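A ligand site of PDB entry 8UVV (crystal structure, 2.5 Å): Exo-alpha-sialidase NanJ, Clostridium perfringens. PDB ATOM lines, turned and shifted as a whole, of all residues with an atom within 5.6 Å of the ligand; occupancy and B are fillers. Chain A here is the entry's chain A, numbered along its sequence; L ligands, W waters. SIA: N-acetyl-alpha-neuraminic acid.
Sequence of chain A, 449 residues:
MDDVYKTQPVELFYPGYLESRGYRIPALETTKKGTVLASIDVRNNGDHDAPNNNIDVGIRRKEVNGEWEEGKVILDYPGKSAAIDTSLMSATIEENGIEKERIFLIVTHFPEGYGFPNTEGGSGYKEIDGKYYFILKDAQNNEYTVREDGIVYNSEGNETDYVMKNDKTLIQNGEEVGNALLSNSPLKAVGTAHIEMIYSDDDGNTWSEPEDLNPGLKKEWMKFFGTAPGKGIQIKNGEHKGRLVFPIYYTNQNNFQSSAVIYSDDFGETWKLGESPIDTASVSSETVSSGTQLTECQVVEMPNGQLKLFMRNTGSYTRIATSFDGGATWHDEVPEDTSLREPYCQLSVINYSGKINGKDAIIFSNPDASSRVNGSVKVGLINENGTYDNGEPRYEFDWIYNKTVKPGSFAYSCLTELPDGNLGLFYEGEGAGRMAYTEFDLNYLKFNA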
ATOM      1  N   ARG A  24     -28.857 -30.256 -16.936  1.00  0.00           N
ATOM      2  CA  ARG A  24     -28.592 -30.811 -18.257  1.00  0.00           C
ATOM      3  C   ARG A  24     -27.267 -31.562 -18.235  1.00  0.00           C
ATOM      4  O   ARG A  24     -26.495 -31.463 -17.284  1.00  0.00           O
ATOM      5  CB  ARG A  24     -28.552 -29.728 -19.343  1.00  0.00           C
ATOM      6  CG  ARG A  24     -29.896 -29.361 -19.949  1.00  0.00           C
ATOM      7  CD  ARG A  24     -29.737 -28.855 -21.368  1.00  0.00           C
ATOM      8  NE  ARG A  24     -29.232 -29.903 -22.239  1.00  0.00           N
ATOM      9  CZ  ARG A  24     -28.920 -29.728 -23.518  1.00  0.00           C
ATOM     10  NH1 ARG A  24     -29.060 -28.556 -24.116  1.00  0.00           N
ATOM     11  NH2 ARG A  24     -28.463 -30.762 -24.218  1.00  0.00           N
ATOM     12  N   ILE A  25     -27.020 -32.293 -19.311  1.00  0.00           N
ATOM     13  CA  ILE A  25     -25.716 -32.875 -19.638  1.00  0.00           C
ATOM     14  C   ILE A  25     -25.393 -34.023 -18.676  1.00  0.00           C
ATOM     15  O   ILE A  25     -24.583 -33.852 -17.750  1.00  0.00           O
ATOM     16  CB  ILE A  25     -24.611 -31.803 -19.638  1.00  0.00           C
ATOM     17  CG1 ILE A  25     -25.070 -30.550 -20.399  1.00  0.00           C
ATOM     18  CG2 ILE A  25     -23.373 -32.331 -20.301  1.00  0.00           C
ATOM     19  CD1 ILE A  25     -25.550 -30.823 -21.799  1.00  0.00           C
ATOM     20  N   ASP A  41     -24.777 -30.936 -15.035  1.00  0.00           N
ATOM     21  CA  ASP A  41     -24.722 -29.483 -14.980  1.00  0.00           C
ATOM     22  C   ASP A  41     -25.768 -28.983 -13.993  1.00  0.00           C
ATOM     23  O   ASP A  41     -26.972 -29.211 -14.182  1.00  0.00           O
ATOM     24  CB  ASP A  41     -24.986 -28.860 -16.357  1.00  0.00           C
ATOM     25  CG  ASP A  41     -23.753 -28.806 -17.230  1.00  0.00           C
ATOM     26  OD1 ASP A  41     -22.787 -29.559 -16.977  1.00  0.00           O
ATOM     27  OD2 ASP A  41     -23.749 -28.002 -18.177  1.00  0.00           O
ATOM     28  N   ARG A  43     -27.370 -26.161 -13.590  1.00  0.00           N
ATOM     29  CA  ARG A  43     -27.668 -24.907 -14.300  1.00  0.00           C
ATOM     30  C   ARG A  43     -28.695 -24.128 -13.484  1.00  0.00           C
ATOM     31  O   ARG A  43     -29.909 -24.241 -13.691  1.00  0.00           O
ATOM     32  CB  ARG A  43     -28.148 -25.215 -15.712  1.00  0.00           C
ATOM     33  CG  ARG A  43     -27.170 -26.035 -16.518  1.00  0.00           C
ATOM     34  CD  ARG A  43     -27.492 -26.038 -18.000  1.00  0.00           C
ATOM     35  NE  ARG A  43     -26.402 -26.646 -18.764  1.00  0.00           N
ATOM     36  CZ  ARG A  43     -26.293 -26.600 -20.077  1.00  0.00           C
ATOM     37  NH1 ARG A  43     -27.201 -25.986 -20.832  1.00  0.00           N
ATOM     38  NH2 ARG A  43     -25.246 -27.162 -20.667  1.00  0.00           N
ATOM     39  N   ASP A  49     -27.522 -22.824 -22.203  1.00  0.00           N
ATOM     40  CA  ASP A  49     -26.075 -22.929 -22.143  1.00  0.00           C
ATOM     41  C   ASP A  49     -25.468 -21.624 -21.613  1.00  0.00           C
ATOM     42  O   ASP A  49     -26.143 -20.596 -21.477  1.00  0.00           O
ATOM     43  CB  ASP A  49     -25.489 -23.225 -23.526  1.00  0.00           C
ATOM     44  CG  ASP A  49     -25.946 -24.566 -24.081  1.00  0.00           C
ATOM     45  OD1 ASP A  49     -26.342 -25.457 -23.295  1.00  0.00           O
ATOM     46  OD2 ASP A  49     -25.894 -24.736 -25.321  1.00  0.00           O
ATOM     47  N   ALA A  50     -24.182 -21.680 -21.314  1.00  0.00           N
ATOM     48  CA  ALA A  50     -23.435 -20.456 -21.060  1.00  0.00           C
ATOM     49  C   ALA A  50     -23.470 -19.592 -22.319  1.00  0.00           C
ATOM     50  O   ALA A  50     -23.530 -20.110 -23.438  1.00  0.00           O
ATOM     51  CB  ALA A  50     -21.989 -20.785 -20.671  1.00  0.00           C
ATOM     52  N   ILE A  84     -19.399 -26.308 -17.269  1.00  0.00           N
ATOM     53  CA  ILE A  84     -20.395 -26.860 -18.176  1.00  0.00           C
ATOM     54  C   ILE A  84     -19.812 -28.071 -18.883  1.00  0.00           C
ATOM     55  O   ILE A  84     -18.640 -28.077 -19.274  1.00  0.00           O
ATOM     56  CB  ILE A  84     -20.857 -25.776 -19.180  1.00  0.00           C
ATOM     57  CG1 ILE A  84     -21.821 -26.343 -20.219  1.00  0.00           C
ATOM     58  CG2 ILE A  84     -19.653 -25.114 -19.848  1.00  0.00           C
ATOM     59  CD1 ILE A  84     -22.328 -25.291 -21.190  1.00  0.00           C
ATOM     60  N   ASP A  85     -20.647 -29.110 -19.042  1.00  0.00           N
ATOM     61  CA  ASP A  85     -20.291 -30.341 -19.747  1.00  0.00           C
ATOM     62  C   ASP A  85     -19.204 -31.118 -18.997  1.00  0.00           C
ATOM     63  O   ASP A  85     -18.010 -30.802 -19.112  1.00  0.00           O
ATOM     64  CB  ASP A  85     -19.842 -30.058 -21.186  1.00  0.00           C
ATOM     65  CG  ASP A  85     -20.924 -29.377 -22.009  1.00  0.00           C
ATOM     66  OD1 ASP A  85     -22.096 -29.384 -21.590  1.00  0.00           O
ATOM     67  OD2 ASP A  85     -20.592 -28.840 -23.084  1.00  0.00           O
ATOM     68  N   THR A 108     -15.691 -28.140 -18.887  1.00  0.00           N
ATOM     69  CA  THR A 108     -15.376 -26.891 -19.548  1.00  0.00           C
ATOM     70  C   THR A 108     -15.726 -25.707 -18.647  1.00  0.00           C
ATOM     71  O   THR A 108     -16.761 -25.715 -17.978  1.00  0.00           O
ATOM     72  CB  THR A 108     -16.136 -26.783 -20.877  1.00  0.00           C
ATOM     73  OG1 THR A 108     -15.999 -28.015 -21.594  1.00  0.00           O
ATOM     74  CG2 THR A 108     -15.594 -25.627 -21.716  1.00  0.00           C
ATOM     75  N   PHE A 110     -15.837 -21.356 -18.310  1.00  0.00           N
ATOM     76  CA  PHE A 110     -15.864 -20.032 -18.884  1.00  0.00           C
ATOM     77  C   PHE A 110     -15.926 -18.981 -17.787  1.00  0.00           C
ATOM     78  O   PHE A 110     -16.592 -19.193 -16.770  1.00  0.00           O
ATOM     79  CB  PHE A 110     -17.076 -19.848 -19.809  1.00  0.00           C
ATOM     80  CG  PHE A 110     -16.969 -20.563 -21.119  1.00  0.00           C
ATOM     81  CD1 PHE A 110     -16.278 -19.997 -22.174  1.00  0.00           C
ATOM     82  CD2 PHE A 110     -17.580 -21.794 -21.296  1.00  0.00           C
ATOM     83  CE1 PHE A 110     -16.188 -20.646 -23.383  1.00  0.00           C
ATOM     84  CE2 PHE A 110     -17.490 -22.454 -22.514  1.00  0.00           C
ATOM     85  CZ  PHE A 110     -16.785 -21.874 -23.555  1.00  0.00           C
ATOM     86  N   PHE A 116     -19.707 -20.845 -25.494  1.00  0.00           N
ATOM     87  CA  PHE A 116     -19.337 -21.277 -26.844  1.00  0.00           C
ATOM     88  C   PHE A 116     -19.568 -20.221 -27.915  1.00  0.00           C
ATOM     89  O   PHE A 116     -18.664 -20.004 -28.734  1.00  0.00           O
ATOM     90  CB  PHE A 116     -20.088 -22.579 -27.181  1.00  0.00           C
ATOM     91  CG  PHE A 116     -19.773 -23.117 -28.552  1.00  0.00           C
ATOM     92  CD1 PHE A 116     -20.474 -22.685 -29.669  1.00  0.00           C
ATOM     93  CD2 PHE A 116     -18.774 -24.067 -28.727  1.00  0.00           C
ATOM     94  CE1 PHE A 116     -20.180 -23.177 -30.935  1.00  0.00           C
ATOM     95  CE2 PHE A 116     -18.483 -24.571 -29.980  1.00  0.00           C
ATOM     96  CZ  PHE A 116     -19.183 -24.127 -31.088  1.00  0.00           C
ATOM     97  N   PHE A 224     -12.968 -22.064 -28.911  1.00  0.00           N
ATOM     98  CA  PHE A 224     -13.565 -23.042 -28.029  1.00  0.00           C
ATOM     99  C   PHE A 224     -12.613 -24.213 -27.829  1.00  0.00           C
ATOM    100  O   PHE A 224     -11.854 -24.578 -28.731  1.00  0.00           O
ATOM    101  CB  PHE A 224     -14.897 -23.556 -28.551  1.00  0.00           C
ATOM    102  CG  PHE A 224     -15.551 -24.558 -27.633  1.00  0.00           C
ATOM    103  CD1 PHE A 224     -16.142 -24.157 -26.451  1.00  0.00           C
ATOM    104  CD2 PHE A 224     -15.544 -25.911 -27.945  1.00  0.00           C
ATOM    105  CE1 PHE A 224     -16.735 -25.066 -25.588  1.00  0.00           C
ATOM    106  CE2 PHE A 224     -16.132 -26.846 -27.095  1.00  0.00           C
ATOM    107  CZ  PHE A 224     -16.731 -26.416 -25.915  1.00  0.00           C
ATOM    108  N   TYR A 249     -13.369 -31.471 -27.764  1.00  0.00           N
ATOM    109  CA  TYR A 249     -13.447 -30.875 -29.092  1.00  0.00           C
ATOM    110  C   TYR A 249     -13.160 -29.385 -28.970  1.00  0.00           C
ATOM    111  O   TYR A 249     -13.196 -28.815 -27.884  1.00  0.00           O
ATOM    112  CB  TYR A 249     -14.797 -31.134 -29.775  1.00  0.00           C
ATOM    113  CG  TYR A 249     -16.017 -30.472 -29.168  1.00  0.00           C
ATOM    114  CD1 TYR A 249     -16.468 -30.820 -27.898  1.00  0.00           C
ATOM    115  CD2 TYR A 249     -16.755 -29.541 -29.885  1.00  0.00           C
ATOM    116  CE1 TYR A 249     -17.600 -30.225 -27.353  1.00  0.00           C
ATOM    117  CE2 TYR A 249     -17.890 -28.944 -29.353  1.00  0.00           C
ATOM    118  CZ  TYR A 249     -18.300 -29.294 -28.084  1.00  0.00           C
ATOM    119  OH  TYR A 249     -19.428 -28.702 -27.547  1.00  0.00           O
ATOM    120  N   GLN A 257     -15.491 -26.697 -35.914  1.00  0.00           N
ATOM    121  CA  GLN A 257     -15.386 -27.625 -34.786  1.00  0.00           C
ATOM    122  C   GLN A 257     -14.679 -28.915 -35.200  1.00  0.00           C
ATOM    123  O   GLN A 257     -14.960 -29.483 -36.258  1.00  0.00           O
ATOM    124  CB  GLN A 257     -16.784 -27.967 -34.254  1.00  0.00           C
ATOM    125  CG  GLN A 257     -17.534 -26.799 -33.648  1.00  0.00           C
ATOM    126  CD  GLN A 257     -18.987 -27.120 -33.364  1.00  0.00           C
ATOM    127  OE1 GLN A 257     -19.345 -27.474 -32.243  1.00  0.00           O
ATOM    128  NE2 GLN A 257     -19.828 -27.017 -34.382  1.00  0.00           N
ATOM    129  N   THR A 295     -17.741 -32.756 -33.602  1.00  0.00           N
ATOM    130  CA  THR A 295     -17.888 -32.024 -32.356  1.00  0.00           C
ATOM    131  C   THR A 295     -17.818 -33.026 -31.211  1.00  0.00           C
ATOM    132  O   THR A 295     -16.818 -33.725 -31.088  1.00  0.00           O
ATOM    133  CB  THR A 295     -19.158 -31.178 -32.365  1.00  0.00           C
ATOM    134  OG1 THR A 295     -20.281 -32.011 -32.072  1.00  0.00           O
ATOM    135  CG2 THR A 295     -19.366 -30.543 -33.751  1.00  0.00           C
ATOM    136  N   GLU A 296     -18.850 -33.090 -30.369  1.00  0.00           N
ATOM    137  CA  GLU A 296     -18.855 -33.984 -29.217  1.00  0.00           C
ATOM    138  C   GLU A 296     -18.603 -35.432 -29.638  1.00  0.00           C
ATOM    139  O   GLU A 296     -19.029 -35.870 -30.710  1.00  0.00           O
ATOM    140  CB  GLU A 296     -20.184 -33.877 -28.470  1.00  0.00           C
ATOM    141  CG  GLU A 296     -20.399 -32.534 -27.795  1.00  0.00           C
ATOM    142  CD  GLU A 296     -21.841 -32.293 -27.400  1.00  0.00           C
ATOM    143  OE1 GLU A 296     -22.751 -32.873 -28.051  1.00  0.00           O
ATOM    144  OE2 GLU A 296     -22.075 -31.531 -26.446  1.00  0.00           O
ATOM    145  N   ARG A 312     -20.451 -36.890 -32.867  1.00  0.00           N
ATOM    146  CA  ARG A 312     -21.500 -36.027 -33.363  1.00  0.00           C
ATOM    147  C   ARG A 312     -20.947 -35.132 -34.468  1.00  0.00           C
ATOM    148  O   ARG A 312     -19.783 -34.708 -34.409  1.00  0.00           O
ATOM    149  CB  ARG A 312     -22.068 -35.199 -32.209  1.00  0.00           C
ATOM    150  CG  ARG A 312     -23.001 -34.046 -32.581  1.00  0.00           C
ATOM    151  CD  ARG A 312     -23.337 -33.227 -31.346  1.00  0.00           C
ATOM    152  NE  ARG A 312     -24.115 -32.022 -31.651  1.00  0.00           N
ATOM    153  CZ  ARG A 312     -24.664 -31.233 -30.746  1.00  0.00           C
ATOM    154  NH1 ARG A 312     -24.551 -31.493 -29.447  1.00  0.00           N
ATOM    155  NH2 ARG A 312     -25.342 -30.161 -31.132  1.00  0.00           N
ATOM    156  N   TYR A 344     -27.381 -34.492 -34.902  1.00  0.00           N
ATOM    157  CA  TYR A 344     -26.608 -33.417 -34.269  1.00  0.00           C
ATOM    158  C   TYR A 344     -26.918 -33.339 -32.786  1.00  0.00           C
ATOM    159  O   TYR A 344     -27.480 -32.348 -32.305  1.00  0.00           O
ATOM    160  CB  TYR A 344     -26.849 -32.070 -34.954  1.00  0.00           C
ATOM    161  CG  TYR A 344     -25.700 -31.103 -34.803  1.00  0.00           C
ATOM    162  CD1 TYR A 344     -24.398 -31.507 -35.081  1.00  0.00           C
ATOM    163  CD2 TYR A 344     -25.908 -29.790 -34.410  1.00  0.00           C
ATOM    164  CE1 TYR A 344     -23.336 -30.626 -34.950  1.00  0.00           C
ATOM    165  CE2 TYR A 344     -24.857 -28.902 -34.275  1.00  0.00           C
ATOM    166  CZ  TYR A 344     -23.572 -29.331 -34.554  1.00  0.00           C
ATOM    167  OH  TYR A 344     -22.522 -28.454 -34.429  1.00  0.00           O
ATOM    168  N   ARG A 372     -34.207 -34.978 -31.949  1.00  0.00           N
ATOM    169  CA  ARG A 372     -33.872 -35.537 -30.648  1.00  0.00           C
ATOM    170  C   ARG A 372     -35.070 -36.284 -30.045  1.00  0.00           C
ATOM    171  O   ARG A 372     -35.624 -35.925 -29.007  1.00  0.00           O
ATOM    172  CB  ARG A 372     -33.374 -34.438 -29.723  1.00  0.00           C
ATOM    173  CG  ARG A 372     -32.134 -33.732 -30.267  1.00  0.00           C
ATOM    174  CD  ARG A 372     -31.554 -32.735 -29.277  1.00  0.00           C
ATOM    175  NE  ARG A 372     -30.291 -32.189 -29.769  1.00  0.00           N
ATOM    176  CZ  ARG A 372     -29.490 -31.397 -29.067  1.00  0.00           C
ATOM    177  NH1 ARG A 372     -29.807 -31.019 -27.836  1.00  0.00           N
ATOM    178  NH2 ARG A 372     -28.350 -30.984 -29.608  1.00  0.00           N
ATOM    179  N   TYR A 412     -29.280 -35.770 -24.684  1.00  0.00           N
ATOM    180  CA  TYR A 412     -28.001 -36.246 -24.185  1.00  0.00           C
ATOM    181  C   TYR A 412     -28.196 -37.461 -23.294  1.00  0.00           C
ATOM    182  O   TYR A 412     -29.132 -37.526 -22.505  1.00  0.00           O
ATOM    183  CB  TYR A 412     -27.287 -35.137 -23.406  1.00  0.00           C
ATOM    184  CG  TYR A 412     -26.595 -34.091 -24.259  1.00  0.00           C
ATOM    185  CD1 TYR A 412     -27.215 -33.567 -25.384  1.00  0.00           C
ATOM    186  CD2 TYR A 412     -25.338 -33.617 -23.918  1.00  0.00           C
ATOM    187  CE1 TYR A 412     -26.598 -32.606 -26.156  1.00  0.00           C
ATOM    188  CE2 TYR A 412     -24.697 -32.659 -24.688  1.00  0.00           C
ATOM    189  CZ  TYR A 412     -25.333 -32.150 -25.805  1.00  0.00           C
ATOM    190  OH  TYR A 412     -24.701 -31.197 -26.566  1.00  0.00           O
HETATM  191  C1  SIA L   1     -26.932 -29.009 -27.424  1.00  0.00           C
HETATM  192  C2  SIA L   1     -25.883 -28.069 -26.693  1.00  0.00           C
HETATM  193  C3  SIA L   1     -25.681 -28.370 -25.192  1.00  0.00           C
HETATM  194  C4  SIA L   1     -24.254 -28.466 -24.662  1.00  0.00           C
HETATM  195  C5  SIA L   1     -23.396 -27.492 -25.461  1.00  0.00           C
HETATM  196  C6  SIA L   1     -23.335 -28.030 -26.910  1.00  0.00           C
HETATM  197  C7  SIA L   1     -22.547 -27.043 -27.810  1.00  0.00           C
HETATM  198  C8  SIA L   1     -22.495 -27.515 -29.284  1.00  0.00           C
HETATM  199  C9  SIA L   1     -21.786 -26.479 -30.148  1.00  0.00           C
HETATM  200  C10 SIA L   1     -21.552 -26.030 -24.714  1.00  0.00           C
HETATM  201  C11 SIA L   1     -20.142 -25.950 -24.118  1.00  0.00           C
HETATM  202  N5  SIA L   1     -22.064 -27.277 -24.903  1.00  0.00           N
HETATM  203  O1A SIA L   1     -27.631 -29.680 -26.623  1.00  0.00           O
HETATM  204  O1B SIA L   1     -26.976 -28.974 -28.674  1.00  0.00           O
HETATM  205  O2  SIA L   1     -26.377 -26.790 -26.857  1.00  0.00           O
HETATM  206  O4  SIA L   1     -24.143 -28.120 -23.272  1.00  0.00           O
HETATM  207  O6  SIA L   1     -24.635 -28.063 -27.496  1.00  0.00           O
HETATM  208  O7  SIA L   1     -23.105 -25.745 -27.683  1.00  0.00           O
HETATM  209  O8  SIA L   1     -21.900 -28.815 -29.367  1.00  0.00           O
HETATM  210  O9  SIA L   1     -22.186 -26.614 -31.513  1.00  0.00           O
HETATM  211  O10 SIA L   1     -22.155 -24.998 -25.011  1.00  0.00           O
HETATM  212  O   HOH W   1     -20.209 -30.163 -25.456  1.00  0.00           O
HETATM  213  O   HOH W   2     -27.391 -27.581 -31.579  1.00  0.00           O
HETATM  214  O   HOH W   3     -21.787 -22.229 -24.081  1.00  0.00           O
HETATM  215  O   HOH W   4     -23.284 -25.618 -34.261  1.00  0.00           O
HETATM  216  O   HOH W   5     -21.930 -29.645 -31.693  1.00  0.00           O
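NH2 of Arg 372 lies within salt-bridge range of O1B of the ligand, at 2.6 Å.
OD2 of Asp 49 is in hydrogen-bond range of O2 of the ligand.
The guanidinium group of Arg 24 lies within salt-bridge range of an oxygen (O1A) of the ligand.
OD2 of Asp 85 lies within hydrogen-bond range of N5 of the ligand (2.8 Å).
The guanidinium group (NH2) of Arg 43 lies within hydrogen-bond range of an oxygen (O4) of the ligand (3.0 Å).
An oxygen (O9) of the ligand sits at hydrogen-bond distance from the side-chain amide oxygen of Gln 257, at 3.1 Å.
OH of Tyr 249 lies within hydrogen-bond range of O8 of the ligand.
O6 of the ligand lies close to OH of Tyr 412 (3.3 Å).
The guanidinium group (NH2) of Arg 312 lies within salt-bridge range of an oxygen (O1B) of the ligand.
An oxygen (O9) of the ligand is in hydrogen-bond range of the side-chain hydroxyl of Tyr 344 (3.5 Å).
The side-chain carboxylate of Asp 85 lies within salt-bridge range of the guanidinium group of Arg 43, 3.96 Å away.
The backbone NH (N) of Asp 85 lies within hydrogen-bond range of the side-chain carboxylate (OD1) of Asp 41, at 3.0 Å.
The side-chain carboxylate of Asp 41 lies within salt-bridge range of the guanidinium group of Arg 43 (3.0 Å).
The side-chain hydroxyl (OH) of Tyr 412 sits at hydrogen-bond distance from the guanidinium group (NH1) of Arg 312.
OH of Tyr 412 is in hydrogen-bond range of OE2 of Glu 296 (2.6 Å).
The backbone carbonyl oxygen (O) of Tyr 344 is in hydrogen-bond range of the guanidinium group (NH2) of Arg 312, at 3.3 Å.
NH1 of Arg 312 is in salt-bridge range of OE1 of Glu 296.
The backbone NH of Thr 295 sits at hydrogen-bond distance from the backbone carbonyl oxygen of Arg 312 (2.9 Å).
Merely in contact with the ligand: Ile 25 (3.4 Å), Phe 116 (3.6 Å), Ile 84 (3.7 Å), Glu 296 (3.7 Å) and Phe 224 (3.8 Å).
Hydrophobic or aromatic side chains within 4 Å of the ligand: Ile 25, Ile 84, Phe 116, Phe 224, Tyr 249 and Tyr 412.
Water W5 lies within hydrogen-bond range of an oxygen (O8) of the ligand, the side-chain hydroxyl of Thr 295, the side-chain hydroxyl of Tyr 344, the guanidinium group of Arg 312 and the side-chain amide oxygen of Gln 257.
Water W3 lies within hydrogen-bond range of the backbone carbonyl oxygen of Ala 50 (2.8 Å), the backbone NH of Phe 116 (2.9 Å) and an oxygen (O10) of the ligand (2.9 Å).
Water W4 bridges OH of Tyr 344 (2.9 Å) and O9 of the ligand (3.1 Å).
Water W2 lies within hydrogen-bond range of an oxygen (O1B) of the ligand (3.2 Å) and the guanidinium group of Arg 312 (3.3 Å).
Water W1 lies within hydrogen-bond range of the side-chain carboxylate (OE2) of Glu 296 (2.5 Å), the side-chain hydroxyl (OH) of Tyr 249 (2.7 Å), the side-chain carboxylate (OD2) of Asp 85 (2.7 Å) and a nitrogen (N5) of the ligand (3.5 Å).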
